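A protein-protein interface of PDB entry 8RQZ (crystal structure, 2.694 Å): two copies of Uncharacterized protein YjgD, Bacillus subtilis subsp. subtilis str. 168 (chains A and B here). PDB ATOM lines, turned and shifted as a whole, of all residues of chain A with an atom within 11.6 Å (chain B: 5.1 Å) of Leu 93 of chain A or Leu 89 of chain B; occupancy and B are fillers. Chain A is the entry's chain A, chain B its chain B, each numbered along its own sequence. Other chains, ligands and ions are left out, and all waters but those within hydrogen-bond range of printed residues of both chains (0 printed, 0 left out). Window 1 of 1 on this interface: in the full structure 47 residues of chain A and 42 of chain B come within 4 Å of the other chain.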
ATOM      1  N   LYS A  84      37.859 -33.992   7.568  1.00  0.00           N
ATOM      2  CA  LYS A  84      37.645 -33.645   6.162  1.00  0.00           C
ATOM      3  C   LYS A  84      36.299 -32.948   5.990  1.00  0.00           C
ATOM      4  O   LYS A  84      36.250 -31.850   5.446  1.00  0.00           O
ATOM      5  CB  LYS A  84      37.721 -34.916   5.289  1.00  0.00           C
ATOM      6  CG  LYS A  84      37.321 -34.736   3.833  1.00  0.00           C
ATOM      7  CD  LYS A  84      37.263 -36.091   3.152  1.00  0.00           C
ATOM      8  CE  LYS A  84      37.493 -36.021   1.666  1.00  0.00           C
ATOM      9  NZ  LYS A  84      37.761 -37.370   1.098  1.00  0.00           N
ATOM     10  N   ASN A  85      35.220 -33.560   6.501  1.00  0.00           N
ATOM     11  CA  ASN A  85      33.877 -32.997   6.408  1.00  0.00           C
ATOM     12  C   ASN A  85      33.645 -31.796   7.317  1.00  0.00           C
ATOM     13  O   ASN A  85      32.730 -31.021   7.060  1.00  0.00           O
ATOM     14  CB  ASN A  85      32.817 -34.070   6.634  1.00  0.00           C
ATOM     15  CG  ASN A  85      32.717 -35.089   5.522  1.00  0.00           C
ATOM     16  OD1 ASN A  85      32.276 -36.221   5.737  1.00  0.00           O
ATOM     17  ND2 ASN A  85      33.099 -34.721   4.302  1.00  0.00           N
ATOM     18  N   LEU A  86      34.459 -31.630   8.362  1.00  0.00           N
ATOM     19  CA  LEU A  86      34.343 -30.471   9.239  1.00  0.00           C
ATOM     20  C   LEU A  86      34.816 -29.233   8.478  1.00  0.00           C
ATOM     21  O   LEU A  86      34.152 -28.204   8.519  1.00  0.00           O
ATOM     22  CB  LEU A  86      35.167 -30.676  10.522  1.00  0.00           C
ATOM     23  CG  LEU A  86      35.256 -29.491  11.478  1.00  0.00           C
ATOM     24  CD1 LEU A  86      33.878 -29.043  11.938  1.00  0.00           C
ATOM     25  CD2 LEU A  86      36.118 -29.831  12.675  1.00  0.00           C
ATOM     26  N   LEU A  87      35.927 -29.349   7.742  1.00  0.00           N
ATOM     27  CA  LEU A  87      36.471 -28.254   6.948  1.00  0.00           C
ATOM     28  C   LEU A  87      35.548 -27.945   5.769  1.00  0.00           C
ATOM     29  O   LEU A  87      35.285 -26.777   5.474  1.00  0.00           O
ATOM     30  CB  LEU A  87      37.866 -28.630   6.440  1.00  0.00           C
ATOM     31  CG  LEU A  87      39.044 -28.052   7.204  1.00  0.00           C
ATOM     32  CD1 LEU A  87      39.160 -28.661   8.592  1.00  0.00           C
ATOM     33  CD2 LEU A  87      40.331 -28.269   6.442  1.00  0.00           C
ATOM     34  N   LEU A  88      35.043 -28.993   5.105  1.00  0.00           N
ATOM     35  CA  LEU A  88      34.129 -28.827   3.977  1.00  0.00           C
ATOM     36  C   LEU A  88      32.796 -28.225   4.416  1.00  0.00           C
ATOM     37  O   LEU A  88      32.174 -27.506   3.639  1.00  0.00           O
ATOM     38  CB  LEU A  88      33.885 -30.164   3.273  1.00  0.00           C
ATOM     39  CG  LEU A  88      35.094 -30.820   2.642  1.00  0.00           C
ATOM     40  CD1 LEU A  88      34.776 -32.236   2.209  1.00  0.00           C
ATOM     41  CD2 LEU A  88      35.627 -29.994   1.501  1.00  0.00           C
ATOM     42  N   LEU A  89      32.364 -28.498   5.659  1.00  0.00           N
ATOM     43  CA  LEU A  89      31.124 -27.956   6.203  1.00  0.00           C
ATOM     44  C   LEU A  89      31.179 -26.430   6.253  1.00  0.00           C
ATOM     45  O   LEU A  89      30.181 -25.776   5.965  1.00  0.00           O
ATOM     46  CB  LEU A  89      30.870 -28.507   7.606  1.00  0.00           C
ATOM     47  CG  LEU A  89      29.439 -28.402   8.069  1.00  0.00           C
ATOM     48  CD1 LEU A  89      28.567 -29.364   7.311  1.00  0.00           C
ATOM     49  CD2 LEU A  89      29.331 -28.623   9.565  1.00  0.00           C
ATOM     50  N   PHE A  90      32.348 -25.865   6.586  1.00  0.00           N
ATOM     51  CA  PHE A  90      32.504 -24.415   6.619  1.00  0.00           C
ATOM     52  C   PHE A  90      32.428 -23.814   5.217  1.00  0.00           C
ATOM     53  O   PHE A  90      31.846 -22.749   5.041  1.00  0.00           O
ATOM     54  CB  PHE A  90      33.782 -24.007   7.361  1.00  0.00           C
ATOM     55  CG  PHE A  90      33.781 -24.480   8.795  1.00  0.00           C
ATOM     56  CD1 PHE A  90      32.641 -24.380   9.575  1.00  0.00           C
ATOM     57  CD2 PHE A  90      34.918 -25.027   9.363  1.00  0.00           C
ATOM     58  CE1 PHE A  90      32.636 -24.832  10.891  1.00  0.00           C
ATOM     59  CE2 PHE A  90      34.908 -25.481  10.680  1.00  0.00           C
ATOM     60  CZ  PHE A  90      33.770 -25.374  11.436  1.00  0.00           C
ATOM     61  N   GLY A  91      32.962 -24.526   4.227  1.00  0.00           N
ATOM     62  CA  GLY A  91      32.901 -24.117   2.828  1.00  0.00           C
ATOM     63  C   GLY A  91      31.483 -24.146   2.286  1.00  0.00           C
ATOM     64  O   GLY A  91      31.102 -23.295   1.477  1.00  0.00           O
ATOM     65  N   THR A  92      30.684 -25.113   2.758  1.00  0.00           N
ATOM     66  CA  THR A  92      29.275 -25.266   2.411  1.00  0.00           C
ATOM     67  C   THR A  92      28.480 -24.100   3.005  1.00  0.00           C
ATOM     68  O   THR A  92      27.660 -23.493   2.317  1.00  0.00           O
ATOM     69  CB  THR A  92      28.774 -26.615   2.924  1.00  0.00           C
ATOM     70  OG1 THR A  92      29.373 -27.647   2.141  1.00  0.00           O
ATOM     71  CG2 THR A  92      27.262 -26.734   2.877  1.00  0.00           C
ATOM     72  N   LEU A  93      28.768 -23.759   4.270  1.00  0.00           N
ATOM     73  CA  LEU A  93      28.150 -22.639   4.981  1.00  0.00           C
ATOM     74  C   LEU A  93      28.484 -21.280   4.326  1.00  0.00           C
ATOM     75  O   LEU A  93      27.673 -20.358   4.369  1.00  0.00           O
ATOM     76  CB  LEU A  93      28.536 -22.662   6.477  1.00  0.00           C
ATOM     77  CG  LEU A  93      27.937 -23.797   7.344  1.00  0.00           C
ATOM     78  CD1 LEU A  93      28.218 -23.572   8.841  1.00  0.00           C
ATOM     79  CD2 LEU A  93      26.430 -23.965   7.119  1.00  0.00           C
ATOM     80  N   GLY A  94      29.646 -21.186   3.687  1.00  0.00           N
ATOM     81  CA  GLY A  94      30.062 -19.992   2.965  1.00  0.00           C
ATOM     82  C   GLY A  94      29.202 -19.733   1.743  1.00  0.00           C
ATOM     83  O   GLY A  94      28.985 -18.579   1.373  1.00  0.00           O
ATOM     84  N   MET A  95      28.689 -20.805   1.115  1.00  0.00           N
ATOM     85  CA  MET A  95      27.800 -20.706  -0.047  1.00  0.00           C
ATOM     86  C   MET A  95      26.372 -20.349   0.396  1.00  0.00           C
ATOM     87  O   MET A  95      25.671 -19.614  -0.298  1.00  0.00           O
ATOM     88  CB  MET A  95      27.758 -22.029  -0.827  1.00  0.00           C
ATOM     89  CG  MET A  95      29.112 -22.552  -1.225  1.00  0.00           C
ATOM     90  SD  MET A  95      28.981 -23.981  -2.338  1.00  0.00           S
ATOM     91  CE  MET A  95      28.249 -25.180  -1.250  1.00  0.00           C
ATOM     92  N   LEU A  96      25.937 -20.913   1.530  1.00  0.00           N
ATOM     93  CA  LEU A  96      24.610 -20.708   2.094  1.00  0.00           C
ATOM     94  C   LEU A  96      24.391 -19.251   2.482  1.00  0.00           C
ATOM     95  O   LEU A  96      25.023 -18.756   3.410  1.00  0.00           O
ATOM     96  CB  LEU A  96      24.435 -21.613   3.319  1.00  0.00           C
ATOM     97  CG  LEU A  96      23.107 -22.335   3.434  1.00  0.00           C
ATOM     98  CD1 LEU A  96      23.291 -23.700   4.062  1.00  0.00           C
ATOM     99  CD2 LEU A  96      22.102 -21.511   4.220  1.00  0.00           C
ATOM    100  N   ASP A  97      23.493 -18.572   1.760  1.00  0.00           N
ATOM    101  CA  ASP A  97      23.105 -17.177   1.951  1.00  0.00           C
ATOM    102  C   ASP A  97      22.280 -17.054   3.229  1.00  0.00           C
ATOM    103  O   ASP A  97      21.051 -17.060   3.178  1.00  0.00           O
ATOM    104  CB  ASP A  97      22.275 -16.707   0.741  1.00  0.00           C
ATOM    105  CG  ASP A  97      22.221 -15.209   0.516  1.00  0.00           C
ATOM    106  OD1 ASP A  97      22.207 -14.457   1.517  1.00  0.00           O
ATOM    107  OD2 ASP A  97      22.168 -14.791  -0.660  1.00  0.00           O
ATOM    108  N   VAL A  98      22.955 -16.945   4.377  1.00  0.00           N
ATOM    109  CA  VAL A  98      22.267 -16.813   5.657  1.00  0.00           C
ATOM    110  C   VAL A  98      21.826 -15.372   5.966  1.00  0.00           C
ATOM    111  O   VAL A  98      21.173 -15.156   6.985  1.00  0.00           O
ATOM    112  CB  VAL A  98      23.094 -17.420   6.803  1.00  0.00           C
ATOM    113  CG1 VAL A  98      23.282 -18.916   6.595  1.00  0.00           C
ATOM    114  CG2 VAL A  98      24.439 -16.729   6.917  1.00  0.00           C
ATOM    115  N   LYS A  99      22.154 -14.399   5.095  1.00  0.00           N
ATOM    116  CA  LYS A  99      21.741 -13.007   5.254  1.00  0.00           C
ATOM    117  C   LYS A  99      20.225 -12.937   5.049  1.00  0.00           C
ATOM    118  O   LYS A  99      19.518 -12.354   5.871  1.00  0.00           O
ATOM    119  CB  LYS A  99      22.468 -12.106   4.228  1.00  0.00           C
ATOM    120  CG  LYS A  99      21.978 -10.658   4.212  1.00  0.00           C
ATOM    121  CD  LYS A  99      22.412  -9.906   2.946  1.00  0.00           C
ATOM    122  CE  LYS A  99      21.807  -8.522   2.859  1.00  0.00           C
ATOM    123  NZ  LYS A  99      22.139  -7.853   1.575  1.00  0.00           N
ATOM    124  N   GLN A 100      19.724 -13.586   3.978  1.00  0.00           N
ATOM    125  CA  GLN A 100      18.298 -13.620   3.646  1.00  0.00           C
ATOM    126  C   GLN A 100      17.489 -14.649   4.447  1.00  0.00           C
ATOM    127  O   GLN A 100      16.306 -14.832   4.175  1.00  0.00           O
ATOM    128  CB  GLN A 100      18.099 -13.837   2.141  1.00  0.00           C
ATOM    129  CG  GLN A 100      18.802 -15.084   1.644  1.00  0.00           C
ATOM    130  CD  GLN A 100      18.608 -15.368   0.178  1.00  0.00           C
ATOM    131  OE1 GLN A 100      18.618 -16.526  -0.231  1.00  0.00           O
ATOM    132  NE2 GLN A 100      18.443 -14.342  -0.658  1.00  0.00           N
ATOM    133  N   LEU A 101      18.108 -15.316   5.423  1.00  0.00           N
ATOM    134  CA  LEU A 101      17.412 -16.274   6.267  1.00  0.00           C
ATOM    135  C   LEU A 101      16.619 -15.580   7.380  1.00  0.00           C
ATOM    136  O   LEU A 101      15.684 -16.180   7.893  1.00  0.00           O
ATOM    137  CB  LEU A 101      18.400 -17.278   6.867  1.00  0.00           C
ATOM    138  CG  LEU A 101      18.282 -18.706   6.353  1.00  0.00           C
ATOM    139  CD1 LEU A 101      18.566 -18.782   4.868  1.00  0.00           C
ATOM    140  CD2 LEU A 101      19.217 -19.620   7.096  1.00  0.00           C
ATOM    141  N   GLU A 102      16.979 -14.326   7.747  1.00  0.00           N
ATOM    142  CA  GLU A 102      16.326 -13.534   8.796  1.00  0.00           C
ATOM    143  C   GLU A 102      14.783 -13.643   8.844  1.00  0.00           C
ATOM    144  O   GLU A 102      14.263 -13.978   9.913  1.00  0.00           O
ATOM    145  CB  GLU A 102      16.747 -12.052   8.732  1.00  0.00           C
ATOM    146  CG  GLU A 102      18.193 -11.766   9.071  1.00  0.00           C
ATOM    147  CD  GLU A 102      18.528 -10.309   8.827  1.00  0.00           C
ATOM    148  OE1 GLU A 102      18.709  -9.936   7.646  1.00  0.00           O
ATOM    149  OE2 GLU A 102      18.577  -9.532   9.808  1.00  0.00           O
ATOM    150  N   LEU A 104      12.724 -15.867   7.310  1.00  0.00           N
ATOM    151  CA  LEU A 104      12.382 -17.290   7.377  1.00  0.00           C
ATOM    152  C   LEU A 104      12.562 -17.844   8.782  1.00  0.00           C
ATOM    153  O   LEU A 104      11.716 -18.597   9.251  1.00  0.00           O
ATOM    154  CB  LEU A 104      13.222 -18.088   6.372  1.00  0.00           C
ATOM    155  CG  LEU A 104      12.960 -19.587   6.320  1.00  0.00           C
ATOM    156  CD1 LEU A 104      11.530 -19.883   5.909  1.00  0.00           C
ATOM    157  CD2 LEU A 104      13.917 -20.264   5.373  1.00  0.00           C
ATOM    158  N   ILE A 105      13.634 -17.436   9.472  1.00  0.00           N
ATOM    159  CA  ILE A 105      13.912 -17.859  10.842  1.00  0.00           C
ATOM    160  C   ILE A 105      12.877 -17.277  11.805  1.00  0.00           C
ATOM    161  O   ILE A 105      12.424 -17.979  12.701  1.00  0.00           O
ATOM    162  CB  ILE A 105      15.375 -17.550  11.245  1.00  0.00           C
ATOM    163  CG1 ILE A 105      16.359 -18.372  10.391  1.00  0.00           C
ATOM    164  CG2 ILE A 105      15.618 -17.788  12.732  1.00  0.00           C
ATOM    165  CD1 ILE A 105      16.201 -19.885  10.510  1.00  0.00           C
ATOM    166  N   ASN B  81      33.285 -15.115   1.690  1.00  0.00           N
ATOM    167  CA  ASN B  81      31.895 -15.521   1.907  1.00  0.00           C
ATOM    168  C   ASN B  81      31.775 -16.498   3.072  1.00  0.00           C
ATOM    169  O   ASN B  81      30.816 -16.426   3.836  1.00  0.00           O
ATOM    170  CB  ASN B  81      31.310 -16.148   0.639  1.00  0.00           C
ATOM    171  CG  ASN B  81      30.603 -15.155  -0.249  1.00  0.00           C
ATOM    172  OD1 ASN B  81      30.118 -14.109   0.209  1.00  0.00           O
ATOM    173  ND2 ASN B  81      30.525 -15.463  -1.540  1.00  0.00           N
ATOM    174  N   ASN B  85      29.405 -15.432   6.183  1.00  0.00           N
ATOM    175  CA  ASN B  85      28.267 -16.244   6.598  1.00  0.00           C
ATOM    176  C   ASN B  85      28.474 -16.957   7.929  1.00  0.00           C
ATOM    177  O   ASN B  85      27.494 -17.344   8.550  1.00  0.00           O
ATOM    178  CB  ASN B  85      27.861 -17.225   5.507  1.00  0.00           C
ATOM    179  CG  ASN B  85      27.248 -16.578   4.283  1.00  0.00           C
ATOM    180  OD1 ASN B  85      27.293 -17.131   3.180  1.00  0.00           O
ATOM    181  ND2 ASN B  85      26.642 -15.406   4.435  1.00  0.00           N
ATOM    182  N   LEU B  86      29.722 -17.128   8.373  1.00  0.00           N
ATOM    183  CA  LEU B  86      29.995 -17.739   9.668  1.00  0.00           C
ATOM    184  C   LEU B  86      29.579 -16.760  10.765  1.00  0.00           C
ATOM    185  O   LEU B  86      28.923 -17.159  11.720  1.00  0.00           O
ATOM    186  CB  LEU B  86      31.480 -18.107   9.799  1.00  0.00           C
ATOM    187  CG  LEU B  86      31.945 -18.623  11.163  1.00  0.00           C
ATOM    188  CD1 LEU B  86      31.180 -19.864  11.577  1.00  0.00           C
ATOM    189  CD2 LEU B  86      33.429 -18.921  11.148  1.00  0.00           C
ATOM    190  N   LEU B  87      29.912 -15.474  10.600  1.00  0.00           N
ATOM    191  CA  LEU B  87      29.549 -14.430  11.555  1.00  0.00           C
ATOM    192  C   LEU B  87      28.036 -14.195  11.532  1.00  0.00           C
ATOM    193  O   LEU B  87      27.411 -14.064  12.584  1.00  0.00           O
ATOM    194  CB  LEU B  87      30.290 -13.135  11.205  1.00  0.00           C
ATOM    195  CG  LEU B  87      31.531 -12.825  12.024  1.00  0.00           C
ATOM    196  CD1 LEU B  87      32.659 -13.789  11.705  1.00  0.00           C
ATOM    197  CD2 LEU B  87      32.001 -11.416  11.772  1.00  0.00           C
ATOM    198  N   LEU B  88      27.455 -14.177  10.322  1.00  0.00           N
ATOM    199  CA  LEU B  88      26.025 -14.011  10.060  1.00  0.00           C
ATOM    200  C   LEU B  88      25.204 -15.181  10.629  1.00  0.00           C
ATOM    201  O   LEU B  88      24.040 -15.000  10.977  1.00  0.00           O
ATOM    202  CB  LEU B  88      25.819 -13.958   8.544  1.00  0.00           C
ATOM    203  CG  LEU B  88      25.468 -12.630   7.895  1.00  0.00           C
ATOM    204  CD1 LEU B  88      26.461 -11.555   8.250  1.00  0.00           C
ATOM    205  CD2 LEU B  88      25.424 -12.780   6.394  1.00  0.00           C
ATOM    206  N   LEU B  89      25.800 -16.382  10.689  1.00  0.00           N
ATOM    207  CA  LEU B  89      25.159 -17.580  11.218  1.00  0.00           C
ATOM    208  C   LEU B  89      24.919 -17.436  12.717  1.00  0.00           C
ATOM    209  O   LEU B  89      23.878 -17.869  13.214  1.00  0.00           O
ATOM    210  CB  LEU B  89      26.026 -18.808  10.951  1.00  0.00           C
ATOM    211  CG  LEU B  89      25.290 -20.124  11.026  1.00  0.00           C
ATOM    212  CD1 LEU B  89      24.357 -20.275   9.853  1.00  0.00           C
ATOM    213  CD2 LEU B  89      26.258 -21.288  11.103  1.00  0.00           C
ATOM    214  N   PHE B  90      25.862 -16.817  13.442  1.00  0.00           N
ATOM    215  CA  PHE B  90      25.695 -16.604  14.875  1.00  0.00           C
ATOM    216  C   PHE B  90      24.586 -15.589  15.159  1.00  0.00           C
ATOM    217  O   PHE B  90      23.826 -15.777  16.106  1.00  0.00           O
ATOM    218  CB  PHE B  90      27.020 -16.217  15.540  1.00  0.00           C
ATOM    219  CG  PHE B  90      28.071 -17.287  15.374  1.00  0.00           C
ATOM    220  CD1 PHE B  90      27.752 -18.625  15.533  1.00  0.00           C
ATOM    221  CD2 PHE B  90      29.376 -16.956  15.056  1.00  0.00           C
ATOM    222  CE1 PHE B  90      28.715 -19.612  15.359  1.00  0.00           C
ATOM    223  CE2 PHE B  90      30.338 -17.946  14.880  1.00  0.00           C
ATOM    224  CZ  PHE B  90      30.002 -19.266  15.037  1.00  0.00           C
ATOM    225  N   GLY B  91      24.459 -14.579  14.304  1.00  0.00           N
ATOM    226  CA  GLY B  91      23.402 -13.580  14.405  1.00  0.00           C
ATOM    227  C   GLY B  91      22.034 -14.175  14.137  1.00  0.00           C
ATOM    228  O   GLY B  91      21.050 -13.778  14.763  1.00  0.00           O
ATOM    229  N   THR B  92      21.973 -15.157  13.224  1.00  0.00           N
ATOM    230  CA  THR B  92      20.760 -15.894  12.878  1.00  0.00           C
ATOM    231  C   THR B  92      20.341 -16.756  14.070  1.00  0.00           C
ATOM    232  O   THR B  92      19.170 -16.763  14.443  1.00  0.00           O
ATOM    233  CB  THR B  92      21.022 -16.736  11.630  1.00  0.00           C
ATOM    234  OG1 THR B  92      21.154 -15.863  10.509  1.00  0.00           O
ATOM    235  CG2 THR B  92      19.929 -17.755  11.369  1.00  0.00           C
ATOM    236  N   LEU B  93      21.315 -17.440  14.695  1.00  0.00           N
ATOM    237  CA  LEU B  93      21.106 -18.271  15.881  1.00  0.00           C
ATOM    238  C   LEU B  93      20.616 -17.438  17.090  1.00  0.00           C
ATOM    239  O   LEU B  93      19.868 -17.947  17.922  1.00  0.00           O
ATOM    240  CB  LEU B  93      22.395 -19.080  16.172  1.00  0.00           C
ATOM    241  CG  LEU B  93      22.886 -19.257  17.602  1.00  0.00           C
ATOM    242  CD1 LEU B  93      22.225 -20.429  18.242  1.00  0.00           C
ATOM    243  CD2 LEU B  93      24.385 -19.431  17.644  1.00  0.00           C
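The backbone carbonyl oxygen of Leu 88 of chain B lies within hydrogen-bond range of the side-chain hydroxyl of Thr 92 of chain B.
Of chain B, only Asn 85 and Leu 89 come within 4 Å of Leu 93 of chain A.
Leu 89 of chain B touches just these residues of chain A: Leu 93 (3.8 Å) and Val 98 (3.7 Å).
Asn 85 of chain B touches just these residues of chain A: Leu 93, Gly 94, Leu 96 and Val 98.
No residue of chain A comes within 4 Å of Leu 86 of chain B.
Gly 91 of chain B touches none of the printed residues of chain A.
Of the printed residues of chain A, Thr 92 of chain B touches Val 98 and Ile 105.
No residue of chain A comes within 4 Å of Leu 93 of chain B.
Of the printed residues of chain B, Lys 99 of chain A touches Leu 88 (3.7 Å).
Of the printed residues of chain B, Leu 96 of chain A touches Asn 85 (2.8 Å).
Of the printed residues of chain B, Gly 94 of chain A touches Asn 81 and Asn 85.
Printed residues of chain B within 4 Å of Val 98 of chain A: Asn 85 (3.5 Å), Leu 88 (3.5 Å), Leu 89 (3.7 Å) and Thr 92 (3.6 Å).
Of the printed residues of chain A, Asn 81 of chain B touches Gly 94.
The nearest printed residue of chain A that does not touch Asn 81 of chain B is Leu 93 of chain A (5.1 Å).
O of Leu 96 of chain A sits close to OD1 of Asn 85 of chain B, 2.8 Å away.
The side-chain amide oxygen (OD1) of Asn 85 of chain B lies close to the backbone carbonyl oxygen (O) of Leu 93 of chain A (3.5 Å).
The backbone carbonyl oxygen (O) of Gly 94 of chain A sits close to the side-chain amide oxygen (OD1) of Asn 85 of chain B (2.9 Å).
Leu 93 of chain A touches Asn 85 of chain B, but with the chains exchanged Asn 85 of chain A does not touch Leu 93 of chain B (17.8 Å).
Leu 93 of chain A touches Leu 89 of chain B, but with the chains exchanged Leu 89 of chain A does not touch Leu 93 of chain B (13.2 Å).
Of the 11 pairs that touch across the chains among the printed residues, none has its exchanged pair printed and touching as well.
Of the 21 printed residues of chain A, 6 touch a printed residue of chain B.
Hydrophobic or aromatic side chains of chain A within 4 Å of the printed part of chain B: Leu 93, Val 98 and Ile 105.
Among the printed residues, no Asp or Glu carboxylate lies within 4 Å of a Lys or Arg side-chain nitrogen of the other chain.
Leu 93 of chain A touches Leu 89 of chain B (CD1 to CD2, 3.8 Å).
Asn 81 of chain B touches Gly 94 of chain A (CB to O, 3.4 Å).
O of Asn 85 of chain B touches CG2 of Val 98 of chain A (3.5 Å).
Leu 88 of chain B touches Val 98 of chain A (CB to CG2, 3.5 Å).
Val 98 of chain A touches Leu 89 of chain B (CG1 to CD1, 3.7 Å).
OG1 of Thr 92 of chain B touches O of Val 98 of chain A (3.6 Å).
Lys 99 of chain A touches Leu 88 of chain B.
Ile 105 of chain A touches Thr 92 of chain B.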
